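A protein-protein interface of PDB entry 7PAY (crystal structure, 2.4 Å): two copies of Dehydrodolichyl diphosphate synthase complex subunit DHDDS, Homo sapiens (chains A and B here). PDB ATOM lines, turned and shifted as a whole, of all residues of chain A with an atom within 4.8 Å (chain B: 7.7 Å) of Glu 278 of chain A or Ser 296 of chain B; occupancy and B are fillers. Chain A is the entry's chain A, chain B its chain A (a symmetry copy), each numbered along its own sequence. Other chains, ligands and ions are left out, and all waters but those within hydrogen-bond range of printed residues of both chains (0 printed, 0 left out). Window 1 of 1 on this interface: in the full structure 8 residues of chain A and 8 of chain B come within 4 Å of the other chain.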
ATOM      1  N   ARG A 274      29.656  20.167  30.903  1.00  0.00           N
ATOM      2  CA  ARG A 274      30.036  21.481  30.396  1.00  0.00           C
ATOM      3  C   ARG A 274      28.836  22.418  30.333  1.00  0.00           C
ATOM      4  O   ARG A 274      28.949  23.604  30.664  1.00  0.00           O
ATOM      5  CB  ARG A 274      30.687  21.346  29.017  1.00  0.00           C
ATOM      6  CG  ARG A 274      31.146  22.661  28.407  1.00  0.00           C
ATOM      7  CD  ARG A 274      31.202  22.583  26.890  1.00  0.00           C
ATOM      8  NE  ARG A 274      29.870  22.496  26.298  1.00  0.00           N
ATOM      9  CZ  ARG A 274      29.280  23.481  25.627  1.00  0.00           C
ATOM     10  NH1 ARG A 274      28.067  23.311  25.126  1.00  0.00           N
ATOM     11  NH2 ARG A 274      29.901  24.639  25.462  1.00  0.00           N
ATOM     12  N   GLN A 275      27.675  21.906  29.919  1.00  0.00           N
ATOM     13  CA  GLN A 275      26.485  22.747  29.869  1.00  0.00           C
ATOM     14  C   GLN A 275      25.977  23.080  31.265  1.00  0.00           C
ATOM     15  O   GLN A 275      25.393  24.150  31.472  1.00  0.00           O
ATOM     16  CB  GLN A 275      25.394  22.067  29.044  1.00  0.00           C
ATOM     17  CG  GLN A 275      25.505  22.339  27.549  1.00  0.00           C
ATOM     18  CD  GLN A 275      24.595  21.454  26.721  1.00  0.00           C
ATOM     19  OE1 GLN A 275      23.405  21.330  27.004  1.00  0.00           O
ATOM     20  NE2 GLN A 275      25.155  20.829  25.692  1.00  0.00           N
ATOM     21  N   GLN A 276      26.190  22.184  32.232  1.00  0.00           N
ATOM     22  CA  GLN A 276      25.842  22.496  33.612  1.00  0.00           C
ATOM     23  C   GLN A 276      26.760  23.567  34.185  1.00  0.00           C
ATOM     24  O   GLN A 276      26.317  24.397  34.990  1.00  0.00           O
ATOM     25  CB  GLN A 276      25.897  21.229  34.468  1.00  0.00           C
ATOM     26  CG  GLN A 276      25.469  21.427  35.917  1.00  0.00           C
ATOM     27  CD  GLN A 276      24.014  21.847  36.050  1.00  0.00           C
ATOM     28  OE1 GLN A 276      23.109  21.141  35.602  1.00  0.00           O
ATOM     29  NE2 GLN A 276      23.784  23.002  36.668  1.00  0.00           N
ATOM     30  N   LEU A 277      28.034  23.571  33.782  1.00  0.00           N
ATOM     31  CA  LEU A 277      28.947  24.618  34.231  1.00  0.00           C
ATOM     32  C   LEU A 277      28.515  25.978  33.706  1.00  0.00           C
ATOM     33  O   LEU A 277      28.509  26.964  34.450  1.00  0.00           O
ATOM     34  CB  LEU A 277      30.375  24.301  33.790  1.00  0.00           C
ATOM     35  N   GLU A 278      28.143  26.047  32.424  1.00  0.00           N
ATOM     36  CA  GLU A 278      27.669  27.305  31.852  1.00  0.00           C
ATOM     37  C   GLU A 278      26.409  27.790  32.554  1.00  0.00           C
ATOM     38  O   GLU A 278      26.267  28.986  32.835  1.00  0.00           O
ATOM     39  CB  GLU A 278      27.412  27.139  30.352  1.00  0.00           C
ATOM     40  CG  GLU A 278      28.649  27.246  29.477  1.00  0.00           C
ATOM     41  CD  GLU A 278      28.493  26.518  28.150  1.00  0.00           C
ATOM     42  OE1 GLU A 278      29.523  26.232  27.505  1.00  0.00           O
ATOM     43  OE2 GLU A 278      27.343  26.228  27.751  1.00  0.00           O
ATOM     44  N   ARG A 279      25.477  26.876  32.841  1.00  0.00           N
ATOM     45  CA  ARG A 279      24.233  27.264  33.498  1.00  0.00           C
ATOM     46  C   ARG A 279      24.500  27.829  34.885  1.00  0.00           C
ATOM     47  O   ARG A 279      23.896  28.831  35.284  1.00  0.00           O
ATOM     48  CB  ARG A 279      23.283  26.066  33.576  1.00  0.00           C
ATOM     49  N   ASP A 280      25.410  27.205  35.632  1.00  0.00           N
ATOM     50  CA  ASP A 280      25.740  27.697  36.964  1.00  0.00           C
ATOM     51  C   ASP A 280      26.628  28.931  36.908  1.00  0.00           C
ATOM     52  O   ASP A 280      26.504  29.815  37.764  1.00  0.00           O
ATOM     53  CB  ASP A 280      26.418  26.595  37.780  1.00  0.00           C
ATOM     54  CG  ASP A 280      25.468  25.473  38.139  1.00  0.00           C
ATOM     55  OD1 ASP A 280      24.295  25.768  38.452  1.00  0.00           O
ATOM     56  OD2 ASP A 280      25.891  24.299  38.107  1.00  0.00           O
ATOM     57  N   GLN A 281      27.527  29.007  35.923  1.00  0.00           N
ATOM     58  CA  GLN A 281      28.334  30.210  35.761  1.00  0.00           C
ATOM     59  C   GLN A 281      27.450  31.422  35.513  1.00  0.00           C
ATOM     60  O   GLN A 281      27.655  32.481  36.116  1.00  0.00           O
ATOM     61  CB  GLN A 281      29.333  30.030  34.619  1.00  0.00           C
ATOM     62  N   ALA A 282      26.446  31.279  34.645  1.00  0.00           N
ATOM     63  CA  ALA A 282      25.530  32.386  34.389  1.00  0.00           C
ATOM     64  C   ALA A 282      24.669  32.697  35.606  1.00  0.00           C
ATOM     65  O   ALA A 282      24.342  33.866  35.846  1.00  0.00           O
ATOM     66  CB  ALA A 282      24.649  32.072  33.180  1.00  0.00           C
ATOM     67  N   THR B 285      26.970  36.465  26.887  1.00  0.00           N
ATOM     68  CA  THR B 285      25.676  36.143  27.485  1.00  0.00           C
ATOM     69  C   THR B 285      24.766  37.365  27.536  1.00  0.00           C
ATOM     70  O   THR B 285      23.548  37.241  27.369  1.00  0.00           O
ATOM     71  CB  THR B 285      25.854  35.561  28.889  1.00  0.00           C
ATOM     72  OG1 THR B 285      26.408  36.558  29.755  1.00  0.00           O
ATOM     73  CG2 THR B 285      26.755  34.332  28.865  1.00  0.00           C
ATOM     74  N   LEU B 293      16.330  34.215  24.637  1.00  0.00           N
ATOM     75  CA  LEU B 293      17.139  33.464  25.586  1.00  0.00           C
ATOM     76  C   LEU B 293      18.002  32.455  24.842  1.00  0.00           C
ATOM     77  O   LEU B 293      17.576  31.884  23.832  1.00  0.00           O
ATOM     78  CB  LEU B 293      16.258  32.746  26.613  1.00  0.00           C
ATOM     79  N   GLN B 294      19.218  32.239  25.344  1.00  0.00           N
ATOM     80  CA  GLN B 294      20.143  31.296  24.729  1.00  0.00           C
ATOM     81  C   GLN B 294      19.643  29.867  24.882  1.00  0.00           C
ATOM     82  O   GLN B 294      19.276  29.226  23.892  1.00  0.00           O
ATOM     83  CB  GLN B 294      21.540  31.433  25.339  1.00  0.00           C
ATOM     84  N   ALA B 295      19.632  29.365  26.121  1.00  0.00           N
ATOM     85  CA  ALA B 295      19.240  27.985  26.416  1.00  0.00           C
ATOM     86  C   ALA B 295      20.037  26.997  25.566  1.00  0.00           C
ATOM     87  O   ALA B 295      19.531  25.958  25.137  1.00  0.00           O
ATOM     88  CB  ALA B 295      17.734  27.785  26.230  1.00  0.00           C
ATOM     89  N   SER B 296      21.302  27.334  25.321  1.00  0.00           N
ATOM     90  CA  SER B 296      22.176  26.561  24.451  1.00  0.00           C
ATOM     91  C   SER B 296      23.454  26.199  25.195  1.00  0.00           C
ATOM     92  O   SER B 296      24.015  27.022  25.928  1.00  0.00           O
ATOM     93  CB  SER B 296      22.515  27.340  23.167  1.00  0.00           C
ATOM     94  N   GLY B 297      23.908  24.965  25.003  1.00  0.00           N
ATOM     95  CA  GLY B 297      23.206  24.018  24.155  1.00  0.00           C
ATOM     96  C   GLY B 297      24.099  23.268  23.188  1.00  0.00           C
ATOM     97  O   GLY B 297      25.311  23.482  23.151  1.00  0.00           O
ATOM     98  N   ASP B 298      23.489  22.384  22.395  1.00  0.00           N
ATOM     99  CA  ASP B 298      24.264  21.563  21.471  1.00  0.00           C
ATOM    100  C   ASP B 298      24.796  22.378  20.297  1.00  0.00           C
ATOM    101  O   ASP B 298      25.888  22.091  19.790  1.00  0.00           O
ATOM    102  CB  ASP B 298      23.414  20.392  20.973  1.00  0.00           C
ATOM    103  CG  ASP B 298      23.052  19.419  22.082  1.00  0.00           C
ATOM    104  OD1 ASP B 298      23.580  19.566  23.202  1.00  0.00           O
ATOM    105  OD2 ASP B 298      22.238  18.505  21.839  1.00  0.00           O
ATOM    106  N   ALA B 299      24.054  23.401  19.864  1.00  0.00           N
ATOM    107  CA  ALA B 299      24.457  24.201  18.713  1.00  0.00           C
ATOM    108  C   ALA B 299      25.711  25.028  18.967  1.00  0.00           C
ATOM    109  O   ALA B 299      26.239  25.612  18.015  1.00  0.00           O
ATOM    110  CB  ALA B 299      23.311  25.121  18.288  1.00  0.00           C
ATOM    111  N   GLN B 300      26.193  25.094  20.212  1.00  0.00           N
ATOM    112  CA  GLN B 300      27.426  25.811  20.554  1.00  0.00           C
ATOM    113  C   GLN B 300      27.370  27.272  20.108  1.00  0.00           C
ATOM    114  O   GLN B 300      28.332  27.807  19.552  1.00  0.00           O
ATOM    115  CB  GLN B 300      28.655  25.111  19.966  1.00  0.00           C
ATOM    116  CG  GLN B 300      29.117  23.890  20.744  1.00  0.00           C
ATOM    117  CD  GLN B 300      30.426  24.128  21.468  1.00  0.00           C
ATOM    118  OE1 GLN B 300      30.489  24.898  22.426  1.00  0.00           O
ATOM    119  NE2 GLN B 300      31.483  23.469  21.009  1.00  0.00           N
ATOM    120  N   LEU B 301      26.229  27.923  20.358  1.00  0.00           N
ATOM    121  CA  LEU B 301      26.051  29.308  19.933  1.00  0.00           C
ATOM    122  C   LEU B 301      27.014  30.237  20.665  1.00  0.00           C
ATOM    123  O   LEU B 301      27.675  31.080  20.046  1.00  0.00           O
ATOM    124  CB  LEU B 301      24.602  29.742  20.159  1.00  0.00           C
ATOM    125  N   ARG B 302      27.107  30.096  21.989  1.00  0.00           N
ATOM    126  CA  ARG B 302      28.035  30.921  22.757  1.00  0.00           C
ATOM    127  C   ARG B 302      29.469  30.742  22.277  1.00  0.00           C
ATOM    128  O   ARG B 302      30.253  31.700  22.292  1.00  0.00           O
ATOM    129  CB  ARG B 302      27.927  30.586  24.245  1.00  0.00           C
ATOM    130  N   ARG B 303      29.828  29.533  21.842  1.00  0.00           N
ATOM    131  CA  ARG B 303      31.192  29.289  21.385  1.00  0.00           C
ATOM    132  C   ARG B 303      31.494  30.063  20.110  1.00  0.00           C
ATOM    133  O   ARG B 303      32.598  30.598  19.950  1.00  0.00           O
ATOM    134  CB  ARG B 303      31.415  27.792  21.171  1.00  0.00           C
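Gly 297 of chain B touches Gln 275 of chain A (C to NE2, 3.7 Å).
Glu 278 of chain A touches Ser 296 of chain B.
NH1 of Arg 274 of chain A lies within hydrogen-bond range of O of Gly 297 of chain B (3.4 Å).
NH2 of Arg 274 of chain A is in hydrogen-bond range of OE1 of Gln 300 of chain B, at 3.1 Å.
The side-chain amide nitrogen (NE2) of Gln 275 of chain A is in hydrogen-bond range of the side-chain carboxylate (OD1) of Asp 298 of chain B, at 3.2 Å.
No position is printed for both chains.
Of the 5 pairs that touch across the chains among the printed residues, none has its exchanged pair printed and touching as well.
Of the printed residues of chain B, Arg 274 of chain A touches Gly 297 (3.4 Å) and Gln 300 (3.1 Å).
Of the printed residues of chain B, Gln 275 of chain A touches Gly 297 (3.7 Å) and Asp 298 (3.2 Å).
No residue of chain B comes within 4 Å of Leu 277 of chain A.
Glu 278 of chain A touches just one residue of chain B: Ser 296.
Leu 293 of chain B touches none of the printed residues of chain A.
Of chain A, only Glu 278 (3.9 Å) comes within 4 Å of Ser 296 of chain B.
Of the printed residues of chain A, Asp 298 of chain B touches Gln 275 (3.2 Å).
Of the printed residues of chain A, Gln 300 of chain B touches Arg 274.
The guanidinium group (NH2) of Arg 274 of chain A lies within salt-bridge range of the side-chain carboxylate (OE1) of Glu 278 of chain A.
Along chain B the printed residues that touch a printed residue of chain A span positions 296 to 300.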
